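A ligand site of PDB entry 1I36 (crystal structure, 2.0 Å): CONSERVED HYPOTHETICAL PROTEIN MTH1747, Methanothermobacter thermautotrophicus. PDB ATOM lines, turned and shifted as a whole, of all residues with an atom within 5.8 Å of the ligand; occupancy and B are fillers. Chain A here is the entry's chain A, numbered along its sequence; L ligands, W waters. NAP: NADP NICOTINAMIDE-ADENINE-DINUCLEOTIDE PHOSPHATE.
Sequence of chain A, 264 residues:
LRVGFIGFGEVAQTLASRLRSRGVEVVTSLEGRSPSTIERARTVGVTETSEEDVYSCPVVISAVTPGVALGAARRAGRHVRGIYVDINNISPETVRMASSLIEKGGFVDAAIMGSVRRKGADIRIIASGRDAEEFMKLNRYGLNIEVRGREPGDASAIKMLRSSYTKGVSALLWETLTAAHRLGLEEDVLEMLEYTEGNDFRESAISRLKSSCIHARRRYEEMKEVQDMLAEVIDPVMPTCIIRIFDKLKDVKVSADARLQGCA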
ATOM      1  N   ILE A   6     -21.204 -16.989  -0.933  1.00  0.00           N
ATOM      2  CA  ILE A   6     -20.324 -16.882  -2.087  1.00  0.00           C
ATOM      3  C   ILE A   6     -20.820 -15.574  -2.695  1.00  0.00           C
ATOM      4  O   ILE A   6     -21.997 -15.478  -3.095  1.00  0.00           O
ATOM      5  CB  ILE A   6     -20.495 -18.033  -3.065  1.00  0.00           C
ATOM      6  CG1 ILE A   6     -20.246 -19.365  -2.367  1.00  0.00           C
ATOM      7  CG2 ILE A   6     -19.497 -17.857  -4.216  1.00  0.00           C
ATOM      8  CD1 ILE A   6     -20.753 -20.576  -3.207  1.00  0.00           C
ATOM      9  N   GLY A   7     -19.937 -14.582  -2.734  1.00  0.00           N
ATOM     10  CA  GLY A   7     -20.277 -13.255  -3.194  1.00  0.00           C
ATOM     11  C   GLY A   7     -20.646 -12.493  -1.934  1.00  0.00           C
ATOM     12  O   GLY A   7     -21.069 -13.102  -0.947  1.00  0.00           O
ATOM     13  N   PHE A   8     -20.371 -11.185  -1.876  1.00  0.00           N
ATOM     14  CA  PHE A   8     -20.777 -10.448  -0.680  1.00  0.00           C
ATOM     15  C   PHE A   8     -21.133  -9.040  -1.042  1.00  0.00           C
ATOM     16  O   PHE A   8     -20.453  -8.084  -0.675  1.00  0.00           O
ATOM     17  CB  PHE A   8     -19.753 -10.538   0.457  1.00  0.00           C
ATOM     18  CG  PHE A   8     -20.353 -10.369   1.825  1.00  0.00           C
ATOM     19  CD1 PHE A   8     -20.816 -11.472   2.529  1.00  0.00           C
ATOM     20  CD2 PHE A   8     -20.507  -9.112   2.376  1.00  0.00           C
ATOM     21  CE1 PHE A   8     -21.454 -11.321   3.775  1.00  0.00           C
ATOM     22  CE2 PHE A   8     -21.133  -8.941   3.613  1.00  0.00           C
ATOM     23  CZ  PHE A   8     -21.605 -10.056   4.315  1.00  0.00           C
ATOM     24  N   GLY A   9     -22.192  -8.949  -1.832  1.00  0.00           N
ATOM     25  CA  GLY A   9     -22.707  -7.688  -2.318  1.00  0.00           C
ATOM     26  C   GLY A   9     -23.915  -7.253  -1.513  1.00  0.00           C
ATOM     27  O   GLY A   9     -23.998  -7.578  -0.332  1.00  0.00           O
ATOM     28  N   GLU A  10     -24.834  -6.550  -2.155  1.00  0.00           N
ATOM     29  CA  GLU A  10     -26.013  -6.029  -1.486  1.00  0.00           C
ATOM     30  C   GLU A  10     -26.927  -7.083  -0.866  1.00  0.00           C
ATOM     31  O   GLU A  10     -27.401  -6.908   0.257  1.00  0.00           O
ATOM     32  CB  GLU A  10     -26.831  -5.140  -2.430  1.00  0.00           C
ATOM     33  CG  GLU A  10     -28.087  -4.603  -1.762  1.00  0.00           C
ATOM     34  CD  GLU A  10     -28.731  -3.449  -2.522  1.00  0.00           C
ATOM     35  OE1 GLU A  10     -28.886  -3.528  -3.755  1.00  0.00           O
ATOM     36  OE2 GLU A  10     -29.109  -2.457  -1.858  1.00  0.00           O
ATOM     37  N   VAL A  11     -27.238  -8.133  -1.624  1.00  0.00           N
ATOM     38  CA  VAL A  11     -28.079  -9.213  -1.101  1.00  0.00           C
ATOM     39  C   VAL A  11     -27.425  -9.906   0.089  1.00  0.00           C
ATOM     40  O   VAL A  11     -28.025 -10.005   1.158  1.00  0.00           O
ATOM     41  CB  VAL A  11     -28.380 -10.239  -2.178  1.00  0.00           C
ATOM     42  CG1 VAL A  11     -29.056 -11.479  -1.579  1.00  0.00           C
ATOM     43  CG2 VAL A  11     -29.251  -9.583  -3.242  1.00  0.00           C
ATOM     44  N   ALA A  12     -26.199 -10.371  -0.100  1.00  0.00           N
ATOM     45  CA  ALA A  12     -25.463 -11.067   0.960  1.00  0.00           C
ATOM     46  C   ALA A  12     -25.350 -10.215   2.225  1.00  0.00           C
ATOM     47  O   ALA A  12     -25.536 -10.703   3.340  1.00  0.00           O
ATOM     48  CB  ALA A  12     -24.053 -11.457   0.459  1.00  0.00           C
ATOM     49  N   GLY A  32      -9.680 -12.257  -3.889  1.00  0.00           N
ATOM     50  CA  GLY A  32     -10.095 -11.896  -5.247  1.00  0.00           C
ATOM     51  C   GLY A  32     -11.253 -10.916  -5.305  1.00  0.00           C
ATOM     52  O   GLY A  32     -11.642 -10.474  -6.394  1.00  0.00           O
ATOM     53  N   ARG A  33     -11.816 -10.566  -4.154  1.00  0.00           N
ATOM     54  CA  ARG A  33     -12.941  -9.635  -4.112  1.00  0.00           C
ATOM     55  C   ARG A  33     -12.478  -8.185  -4.060  1.00  0.00           C
ATOM     56  O   ARG A  33     -11.410  -7.865  -3.554  1.00  0.00           O
ATOM     57  CB  ARG A  33     -13.868  -9.952  -2.926  1.00  0.00           C
ATOM     58  CG  ARG A  33     -14.325 -11.420  -2.874  1.00  0.00           C
ATOM     59  CD  ARG A  33     -15.503 -11.731  -3.832  1.00  0.00           C
ATOM     60  NE  ARG A  33     -15.214 -11.486  -5.243  1.00  0.00           N
ATOM     61  CZ  ARG A  33     -14.617 -12.348  -6.073  1.00  0.00           C
ATOM     62  NH1 ARG A  33     -14.227 -13.547  -5.650  1.00  0.00           N
ATOM     63  NH2 ARG A  33     -14.426 -12.007  -7.344  1.00  0.00           N
ATOM     64  N   SER A  34     -13.330  -7.312  -4.598  1.00  0.00           N
ATOM     65  CA  SER A  34     -13.093  -5.878  -4.657  1.00  0.00           C
ATOM     66  C   SER A  34     -13.184  -5.188  -3.280  1.00  0.00           C
ATOM     67  O   SER A  34     -13.757  -5.730  -2.323  1.00  0.00           O
ATOM     68  CB  SER A  34     -14.145  -5.236  -5.550  1.00  0.00           C
ATOM     69  OG  SER A  34     -15.334  -5.017  -4.804  1.00  0.00           O
ATOM     70  N   SER A  36     -15.017  -2.643  -2.269  1.00  0.00           N
ATOM     71  CA  SER A  36     -16.403  -2.447  -1.819  1.00  0.00           C
ATOM     72  C   SER A  36     -16.974  -3.711  -1.172  1.00  0.00           C
ATOM     73  O   SER A  36     -17.727  -3.633  -0.189  1.00  0.00           O
ATOM     74  CB  SER A  36     -17.307  -1.943  -2.965  1.00  0.00           C
ATOM     75  OG  SER A  36     -17.516  -2.903  -3.996  1.00  0.00           O
ATOM     76  N   THR A  37     -16.580  -4.874  -1.676  1.00  0.00           N
ATOM     77  CA  THR A  37     -17.029  -6.151  -1.120  1.00  0.00           C
ATOM     78  C   THR A  37     -16.348  -6.430   0.221  1.00  0.00           C
ATOM     79  O   THR A  37     -17.006  -6.877   1.169  1.00  0.00           O
ATOM     80  CB  THR A  37     -16.780  -7.305  -2.123  1.00  0.00           C
ATOM     81  OG1 THR A  37     -17.677  -7.174  -3.239  1.00  0.00           O
ATOM     82  CG2 THR A  37     -16.987  -8.670  -1.462  1.00  0.00           C
ATOM     83  N   ARG A  40     -18.047  -4.179   2.737  1.00  0.00           N
ATOM     84  CA  ARG A  40     -19.360  -4.633   3.199  1.00  0.00           C
ATOM     85  C   ARG A  40     -19.172  -5.751   4.237  1.00  0.00           C
ATOM     86  O   ARG A  40     -19.818  -5.757   5.280  1.00  0.00           O
ATOM     87  CB  ARG A  40     -20.192  -5.192   2.045  1.00  0.00           C
ATOM     88  CG  ARG A  40     -20.653  -4.210   1.010  1.00  0.00           C
ATOM     89  CD  ARG A  40     -21.333  -5.072  -0.067  1.00  0.00           C
ATOM     90  NE  ARG A  40     -21.749  -4.334  -1.246  1.00  0.00           N
ATOM     91  CZ  ARG A  40     -22.814  -3.539  -1.285  1.00  0.00           C
ATOM     92  NH1 ARG A  40     -23.561  -3.369  -0.208  1.00  0.00           N
ATOM     93  NH2 ARG A  40     -23.118  -2.906  -2.409  1.00  0.00           N
ATOM     94  N   SER A  62     -25.266 -18.608  -2.630  1.00  0.00           N
ATOM     95  CA  SER A  62     -24.587 -18.007  -3.775  1.00  0.00           C
ATOM     96  C   SER A  62     -25.376 -16.751  -4.163  1.00  0.00           C
ATOM     97  O   SER A  62     -26.499 -16.851  -4.635  1.00  0.00           O
ATOM     98  CB  SER A  62     -24.608 -18.979  -4.956  1.00  0.00           C
ATOM     99  OG  SER A  62     -24.075 -18.360  -6.120  1.00  0.00           O
ATOM    100  N   ALA A  63     -24.773 -15.588  -3.954  1.00  0.00           N
ATOM    101  CA  ALA A  63     -25.405 -14.313  -4.250  1.00  0.00           C
ATOM    102  C   ALA A  63     -24.347 -13.484  -4.998  1.00  0.00           C
ATOM    103  O   ALA A  63     -23.765 -12.538  -4.460  1.00  0.00           O
ATOM    104  CB  ALA A  63     -25.805 -13.604  -2.947  1.00  0.00           C
ATOM    105  N   VAL A  64     -24.012 -13.966  -6.184  1.00  0.00           N
ATOM    106  CA  VAL A  64     -22.992 -13.323  -7.021  1.00  0.00           C
ATOM    107  C   VAL A  64     -23.726 -12.553  -8.116  1.00  0.00           C
ATOM    108  O   VAL A  64     -24.692 -11.864  -7.810  1.00  0.00           O
ATOM    109  CB  VAL A  64     -22.029 -14.400  -7.605  1.00  0.00           C
ATOM    110  CG1 VAL A  64     -21.187 -14.961  -6.473  1.00  0.00           C
ATOM    111  CG2 VAL A  64     -22.835 -15.545  -8.251  1.00  0.00           C
ATOM    112  N   THR A  65     -23.268 -12.590  -9.359  1.00  0.00           N
ATOM    113  CA  THR A  65     -23.997 -11.899 -10.437  1.00  0.00           C
ATOM    114  C   THR A  65     -24.518 -12.993 -11.394  1.00  0.00           C
ATOM    115  O   THR A  65     -24.017 -14.114 -11.401  1.00  0.00           O
ATOM    116  CB  THR A  65     -23.080 -10.894 -11.189  1.00  0.00           C
ATOM    117  OG1 THR A  65     -22.012 -11.595 -11.814  1.00  0.00           O
ATOM    118  CG2 THR A  65     -22.512  -9.894 -10.207  1.00  0.00           C
ATOM    119  N   PRO A  66     -25.559 -12.688 -12.196  1.00  0.00           N
ATOM    120  CA  PRO A  66     -26.055 -13.738 -13.095  1.00  0.00           C
ATOM    121  C   PRO A  66     -24.992 -14.388 -14.007  1.00  0.00           C
ATOM    122  O   PRO A  66     -25.018 -15.611 -14.209  1.00  0.00           O
ATOM    123  CB  PRO A  66     -27.116 -13.008 -13.911  1.00  0.00           C
ATOM    124  CG  PRO A  66     -27.702 -12.051 -12.886  1.00  0.00           C
ATOM    125  CD  PRO A  66     -26.424 -11.488 -12.253  1.00  0.00           C
ATOM    126  N   VAL A  68     -22.007 -15.016 -13.435  1.00  0.00           N
ATOM    127  CA  VAL A  68     -21.015 -15.777 -12.653  1.00  0.00           C
ATOM    128  C   VAL A  68     -21.643 -16.997 -11.929  1.00  0.00           C
ATOM    129  O   VAL A  68     -20.921 -17.844 -11.427  1.00  0.00           O
ATOM    130  CB  VAL A  68     -20.404 -14.791 -11.552  1.00  0.00           C
ATOM    131  CG1 VAL A  68     -19.659 -15.532 -10.469  1.00  0.00           C
ATOM    132  CG2 VAL A  68     -19.486 -13.770 -12.229  1.00  0.00           C
ATOM    133  N   ALA A  72     -19.697 -20.294 -10.312  1.00  0.00           N
ATOM    134  CA  ALA A  72     -19.664 -20.401  -8.863  1.00  0.00           C
ATOM    135  C   ALA A  72     -20.162 -21.783  -8.449  1.00  0.00           C
ATOM    136  O   ALA A  72     -19.610 -22.391  -7.558  1.00  0.00           O
ATOM    137  CB  ALA A  72     -20.538 -19.309  -8.234  1.00  0.00           C
ATOM    138  N   ARG A  75     -17.568 -24.566  -9.136  1.00  0.00           N
ATOM    139  CA  ARG A  75     -16.538 -24.574  -8.100  1.00  0.00           C
ATOM    140  C   ARG A  75     -17.026 -25.089  -6.752  1.00  0.00           C
ATOM    141  O   ARG A  75     -16.346 -25.886  -6.101  1.00  0.00           O
ATOM    142  CB  ARG A  75     -15.946 -23.185  -7.885  1.00  0.00           C
ATOM    143  CG  ARG A  75     -15.031 -22.730  -9.003  1.00  0.00           C
ATOM    144  CD  ARG A  75     -14.377 -21.405  -8.673  1.00  0.00           C
ATOM    145  NE  ARG A  75     -15.336 -20.311  -8.727  1.00  0.00           N
ATOM    146  CZ  ARG A  75     -15.711 -19.679  -9.836  1.00  0.00           C
ATOM    147  NH1 ARG A  75     -15.204 -20.026 -11.010  1.00  0.00           N
ATOM    148  NH2 ARG A  75     -16.647 -18.725  -9.787  1.00  0.00           N
ATOM    149  N   ILE A  87     -29.470 -17.756  -5.235  1.00  0.00           N
ATOM    150  CA  ILE A  87     -30.421 -16.662  -5.197  1.00  0.00           C
ATOM    151  C   ILE A  87     -30.160 -15.676  -6.345  1.00  0.00           C
ATOM    152  O   ILE A  87     -30.732 -14.600  -6.390  1.00  0.00           O
ATOM    153  CB  ILE A  87     -30.401 -15.991  -3.793  1.00  0.00           C
ATOM    154  CG1 ILE A  87     -31.729 -15.294  -3.504  1.00  0.00           C
ATOM    155  CG2 ILE A  87     -29.204 -15.026  -3.655  1.00  0.00           C
ATOM    156  CD1 ILE A  87     -31.925 -14.981  -1.999  1.00  0.00           C
ATOM    157  N   ASN A  88     -29.409 -16.114  -7.336  1.00  0.00           N
ATOM    158  CA  ASN A  88     -29.089 -15.256  -8.479  1.00  0.00           C
ATOM    159  C   ASN A  88     -30.234 -15.106  -9.491  1.00  0.00           C
ATOM    160  O   ASN A  88     -31.059 -16.007  -9.665  1.00  0.00           O
ATOM    161  CB  ASN A  88     -27.834 -15.751  -9.188  1.00  0.00           C
ATOM    162  CG  ASN A  88     -26.644 -15.854  -8.254  1.00  0.00           C
ATOM    163  OD1 ASN A  88     -26.118 -14.864  -7.781  1.00  0.00           O
ATOM    164  ND2 ASN A  88     -26.233 -17.090  -7.958  1.00  0.00           N
ATOM    165  N   ASN A  89     -30.255 -13.974 -10.178  1.00  0.00           N
ATOM    166  CA  ASN A  89     -31.307 -13.754 -11.176  1.00  0.00           C
ATOM    167  C   ASN A  89     -30.913 -14.412 -12.480  1.00  0.00           C
ATOM    168  O   ASN A  89     -30.346 -13.769 -13.349  1.00  0.00           O
ATOM    169  CB  ASN A  89     -31.576 -12.259 -11.399  1.00  0.00           C
ATOM    170  CG  ASN A  89     -32.725 -12.019 -12.375  1.00  0.00           C
ATOM    171  OD1 ASN A  89     -33.680 -12.813 -12.447  1.00  0.00           O
ATOM    172  ND2 ASN A  89     -32.611 -10.944 -13.171  1.00  0.00           N
ATOM    173  N   ILE A 112     -35.942 -13.899  -4.724  1.00  0.00           N
ATOM    174  CA  ILE A 112     -36.274 -12.701  -3.971  1.00  0.00           C
ATOM    175  C   ILE A 112     -37.508 -12.095  -4.657  1.00  0.00           C
ATOM    176  O   ILE A 112     -37.469 -11.806  -5.849  1.00  0.00           O
ATOM    177  CB  ILE A 112     -35.091 -11.706  -3.976  1.00  0.00           C
ATOM    178  CG1 ILE A 112     -33.958 -12.299  -3.114  1.00  0.00           C
ATOM    179  CG2 ILE A 112     -35.521 -10.357  -3.359  1.00  0.00           C
ATOM    180  CD1 ILE A 112     -32.648 -11.484  -3.132  1.00  0.00           C
ATOM    181  N   GLY A 114     -39.134  -9.153  -4.187  1.00  0.00           N
ATOM    182  CA  GLY A 114     -39.330  -7.758  -3.889  1.00  0.00           C
ATOM    183  C   GLY A 114     -38.053  -6.948  -4.018  1.00  0.00           C
ATOM    184  O   GLY A 114     -37.144  -7.307  -4.773  1.00  0.00           O
ATOM    185  N   SER A 115     -38.010  -5.845  -3.280  1.00  0.00           N
ATOM    186  CA  SER A 115     -36.866  -4.936  -3.295  1.00  0.00           C
ATOM    187  C   SER A 115     -35.987  -5.115  -2.057  1.00  0.00           C
ATOM    188  O   SER A 115     -36.426  -4.830  -0.953  1.00  0.00           O
ATOM    189  CB  SER A 115     -37.359  -3.484  -3.370  1.00  0.00           C
ATOM    190  OG  SER A 115     -36.302  -2.562  -3.160  1.00  0.00           O
ATOM    191  N   VAL A 116     -34.761  -5.590  -2.244  1.00  0.00           N
ATOM    192  CA  VAL A 116     -33.848  -5.771  -1.124  1.00  0.00           C
ATOM    193  C   VAL A 116     -33.628  -4.399  -0.464  1.00  0.00           C
ATOM    194  O   VAL A 116     -33.692  -4.263   0.756  1.00  0.00           O
ATOM    195  CB  VAL A 116     -32.479  -6.342  -1.596  1.00  0.00           C
ATOM    196  CG1 VAL A 116     -31.512  -6.432  -0.449  1.00  0.00           C
ATOM    197  CG2 VAL A 116     -32.681  -7.747  -2.176  1.00  0.00           C
ATOM    198  N   ARG A 117     -33.427  -3.395  -1.322  1.00  0.00           N
ATOM    199  CA  ARG A 117     -33.202  -1.999  -0.939  1.00  0.00           C
ATOM    200  C   ARG A 117     -34.296  -1.429  -0.058  1.00  0.00           C
ATOM    201  O   ARG A 117     -34.009  -0.751   0.927  1.00  0.00           O
ATOM    202  CB  ARG A 117     -33.104  -1.149  -2.204  1.00  0.00           C
ATOM    203  CG  ARG A 117     -32.790   0.316  -1.996  1.00  0.00           C
ATOM    204  CD  ARG A 117     -31.304   0.557  -1.677  1.00  0.00           C
ATOM    205  NE  ARG A 117     -30.352  -0.008  -2.639  1.00  0.00           N
ATOM    206  CZ  ARG A 117     -30.432   0.058  -3.979  1.00  0.00           C
ATOM    207  NH1 ARG A 117     -31.443   0.674  -4.576  1.00  0.00           N
ATOM    208  NH2 ARG A 117     -29.466  -0.467  -4.713  1.00  0.00           N
ATOM    209  N   LYS A 159     -41.194 -16.453  -9.952  1.00  0.00           N
ATOM    210  CA  LYS A 159     -40.796 -15.045  -9.886  1.00  0.00           C
ATOM    211  C   LYS A 159     -40.882 -14.361 -11.259  1.00  0.00           C
ATOM    212  O   LYS A 159     -41.423 -13.243 -11.399  1.00  0.00           O
ATOM    213  CB  LYS A 159     -39.372 -14.927  -9.360  1.00  0.00           C
ATOM    214  CG  LYS A 159     -38.858 -13.479  -9.330  1.00  0.00           C
ATOM    215  CD  LYS A 159     -37.443 -13.393  -8.857  1.00  0.00           C
ATOM    216  CE  LYS A 159     -36.895 -11.997  -9.122  1.00  0.00           C
ATOM    217  NZ  LYS A 159     -36.858 -11.779 -10.597  1.00  0.00           N
HETATM  218  PA  NAP L   1     -23.671  -6.944  -6.048  1.00  0.00           P
HETATM  219  O1A NAP L   1     -23.694  -7.110  -7.484  1.00  0.00           O
HETATM  220  O2A NAP L   1     -24.457  -6.204  -5.074  1.00  0.00           O
HETATM  221  O5B NAP L   1     -22.956  -8.261  -5.304  1.00  0.00           O
HETATM  222  C5B NAP L   1     -22.395  -9.547  -5.947  1.00  0.00           C
HETATM  223  C4B NAP L   1     -21.110  -9.557  -5.267  1.00  0.00           C
HETATM  224  O4B NAP L   1     -20.612 -10.966  -5.900  1.00  0.00           O
HETATM  225  C3B NAP L   1     -20.011  -9.133  -5.668  1.00  0.00           C
HETATM  226  O3B NAP L   1     -19.994  -8.614  -4.401  1.00  0.00           O
HETATM  227  C2B NAP L   1     -18.657  -9.551  -6.099  1.00  0.00           C
HETATM  228  O2B NAP L   1     -17.489  -9.402  -5.651  1.00  0.00           O
HETATM  229  C1B NAP L   1     -19.150 -10.867  -6.091  1.00  0.00           C
HETATM  230  N9A NAP L   1     -18.687 -11.635  -7.257  1.00  0.00           N
HETATM  231  C8A NAP L   1     -18.581 -11.465  -8.640  1.00  0.00           C
HETATM  232  N7A NAP L   1     -17.996 -12.489  -9.213  1.00  0.00           N
HETATM  233  C5A NAP L   1     -17.702 -13.371  -8.199  1.00  0.00           C
HETATM  234  C6A NAP L   1     -17.071 -14.664  -8.175  1.00  0.00           C
HETATM  235  N6A NAP L   1     -16.618 -15.248  -9.293  1.00  0.00           N
HETATM  236  N1A NAP L   1     -16.933 -15.295  -6.955  1.00  0.00           N
HETATM  237  C2A NAP L   1     -17.387 -14.714  -5.804  1.00  0.00           C
HETATM  238  N3A NAP L   1     -17.981 -13.506  -5.752  1.00  0.00           N
HETATM  239  C4A NAP L   1     -18.117 -12.891  -7.002  1.00  0.00           C
HETATM  240  O3  NAP L   1     -25.046  -7.848  -6.336  1.00  0.00           O
HETATM  241  PN  NAP L   1     -26.490  -8.131  -5.477  1.00  0.00           P
HETATM  242  O1N NAP L   1     -27.397  -6.961  -5.667  1.00  0.00           O
HETATM  243  O2N NAP L   1     -26.005  -8.449  -4.121  1.00  0.00           O
HETATM  244  O5D NAP L   1     -27.225  -9.430  -5.999  1.00  0.00           O
HETATM  245  C5D NAP L   1     -26.619 -10.739  -5.905  1.00  0.00           C
HETATM  246  C4D NAP L   1     -27.463 -11.716  -6.709  1.00  0.00           C
HETATM  247  O4D NAP L   1     -28.875 -11.787  -6.350  1.00  0.00           O
HETATM  248  C3D NAP L   1     -27.490 -11.450  -8.230  1.00  0.00           C
HETATM  249  O3D NAP L   1     -27.433 -12.634  -9.087  1.00  0.00           O
HETATM  250  C2D NAP L   1     -28.749 -10.682  -8.486  1.00  0.00           C
HETATM  251  O2D NAP L   1     -29.224 -10.805  -9.797  1.00  0.00           O
HETATM  252  C1D NAP L   1     -29.686 -11.259  -7.408  1.00  0.00           C
HETATM  253  N1N NAP L   1     -30.752 -10.343  -6.977  1.00  0.00           N
HETATM  254  C2N NAP L   1     -30.438  -9.098  -6.409  1.00  0.00           C
HETATM  255  C3N NAP L   1     -31.562  -8.286  -6.015  1.00  0.00           C
HETATM  256  C7N NAP L   1     -31.377  -6.979  -5.412  1.00  0.00           C
HETATM  257  O7N NAP L   1     -32.357  -6.292  -5.067  1.00  0.00           O
HETATM  258  N7N NAP L   1     -30.142  -6.463  -5.183  1.00  0.00           N
HETATM  259  C4N NAP L   1     -32.876  -8.769  -6.216  1.00  0.00           C
HETATM  260  C5N NAP L   1     -33.146  -9.969  -6.776  1.00  0.00           C
HETATM  261  C6N NAP L   1     -32.097 -10.760  -7.150  1.00  0.00           C
HETATM  262  P2B NAP L   1     -16.705  -8.112  -6.326  1.00  0.00           P
HETATM  263  O1X NAP L   1     -17.289  -6.830  -5.791  1.00  0.00           O
HETATM  264  O2X NAP L   1     -15.376  -8.376  -5.842  1.00  0.00           O
HETATM  265  O3X NAP L   1     -16.940  -8.193  -7.744  1.00  0.00           O
HETATM  266  O   HOH W   1     -17.098 -18.479  -6.858  1.00  0.00           O
HETATM  267  O   HOH W   2     -15.752  -9.921  -9.505  1.00  0.00           O
HETATM  268  O   HOH W   3     -28.001  -6.519  -8.368  1.00  0.00           O
HETATM  269  O   HOH W   4     -24.651 -10.392  -2.733  1.00  0.00           O
HETATM  270  O   HOH W   5     -13.013  -8.183  -7.493  1.00  0.00           O
HETATM  271  O   HOH W   6     -13.909 -15.931  -7.244  1.00  0.00           O
HETATM  272  O   HOH W   7     -27.269  -4.240  -6.095  1.00  0.00           O
HETATM  273  O   HOH W   8     -19.255  -8.134  -9.699  1.00  0.00           O
HETATM  274  O   HOH W   9     -28.648  -8.822 -11.392  1.00  0.00           O
HETATM  275  O   HOH W  10     -25.792  -8.548  -9.643  1.00  0.00           O
HETATM  276  O   HOH W  11     -32.635  -3.499  -4.489  1.00  0.00           O
HETATM  277  O   HOH W  12     -31.689  -8.956 -10.106  1.00  0.00           O
HETATM  278  O   HOH W  13     -17.526 -15.133  -2.664  1.00  0.00           O
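An oxygen (O4D) of the ligand lies close to the backbone carbonyl oxygen (O) of Ile 87 (3.4 Å). Gly 7 touches the ligand (CA to N3A, 3.4 Å). Phe 8 touches the ligand (C to O3B, 3.6 Å). O of Ala 63 touches C5B of the ligand, at 3.6 Å. Thr 65 touches the ligand (C to O3D, 3.7 Å). CD of Pro 66 touches O3D of the ligand, 3.5 Å away. Val 68 touches the ligand. Arg 75 touches the ligand. Ile 112 touches the ligand (CB to C5N, 3.8 Å). Val 116 touches the ligand. Hydrophobic or aromatic side chains within 4 Å of the ligand: Val 11, Val 64, Pro 66, Val 68, Ile 112 and Val 116. 19 residues have an atom within 4 Å of the ligand: Gly 7, Phe 8, Gly 9, Glu 10, Val 11, Arg 33, Ser 34, Thr 37, Ala 63, Val 64, Thr 65, Pro 66, Val 68, Arg 75, Ile 87, Asn 88, Asn 89, Ile 112 and Val 116. The nearest printed residue that does not touch the ligand is Ile 6 (4.1 Å).
O1X of the ligand sits at hydrogen-bond distance from OG1 of Thr 37, at 2.6 Å. The backbone NH (N) of Ser 34 is in hydrogen-bond range of an oxygen (O2X) of the ligand, 2.6 Å away. O1X of the ligand is in hydrogen-bond range of OG of Ser 34 (2.8 Å). N of Val 11 lies within hydrogen-bond range of O2N of the ligand (2.8 Å). The backbone carbonyl oxygen of Val 64 sits close to an oxygen (O3D) of the ligand, 3.1 Å away. The side-chain amide oxygen (OD1) of Asn 88 sits at hydrogen-bond distance from an oxygen (O3D) of the ligand. An oxygen (O2A) of the ligand is in hydrogen-bond range of the backbone NH of Glu 10 (3.0 Å). The side-chain carboxylate (OE1) of Glu 10 lies within hydrogen-bond range of a nitrogen (N7N) of the ligand (3.5 Å). An oxygen (O3B) of the ligand lies within hydrogen-bond range of the backbone NH of Gly 9 (3.4 Å). An oxygen (O2X) of the ligand is in salt-bridge range of the guanidinium group (NE) of Arg 33, at 3.2 Å. N of Asn 89 sits at hydrogen-bond distance from O3D of the ligand, at 3.3 Å.
The side-chain hydroxyl (OG) of Ser 34 is in hydrogen-bond range of the backbone NH (N) of Thr 37 (3.4 Å). The side-chain hydroxyl of Ser 36 lies within hydrogen-bond range of the side-chain hydroxyl of Ser 34 (3.1 Å). N of Val 64 is in hydrogen-bond range of OD1 of Asn 88 (2.8 Å). ND2 of Asn 88 sits at hydrogen-bond distance from OG of Ser 62, at 3.1 Å. NE of Arg 117 lies within salt-bridge range of OE2 of Glu 10 (2.9 Å). O of Ser 62 is in hydrogen-bond range of N of Ile 87 (3.2 Å). The backbone NH (N) of Ala 63 lies within hydrogen-bond range of the backbone carbonyl oxygen (O) of Ile 6 (2.9 Å).
Water W2 bridges O3X of the ligand and NH2 of Arg 33. Water W4 lies within hydrogen-bond range of an oxygen (O2N) of the ligand, the backbone carbonyl oxygen of Ala 63, the backbone NH of Gly 9 and the backbone NH of Ala 12. Water W7 lies within hydrogen-bond range of O1N of the ligand (2.8 Å) and OE1 of Glu 10 (2.9 Å). Water W5 lies within hydrogen-bond range of O of Gly 32, O2X of the ligand and N of Ser 34. Water W6 bridges NH1 of Arg 33 (2.9 Å) and N1A of the ligand (3.1 Å). Water W1 lies within hydrogen-bond range of NH2 of Arg 75 (3.0 Å) and N1A of the ligand (3.2 Å).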
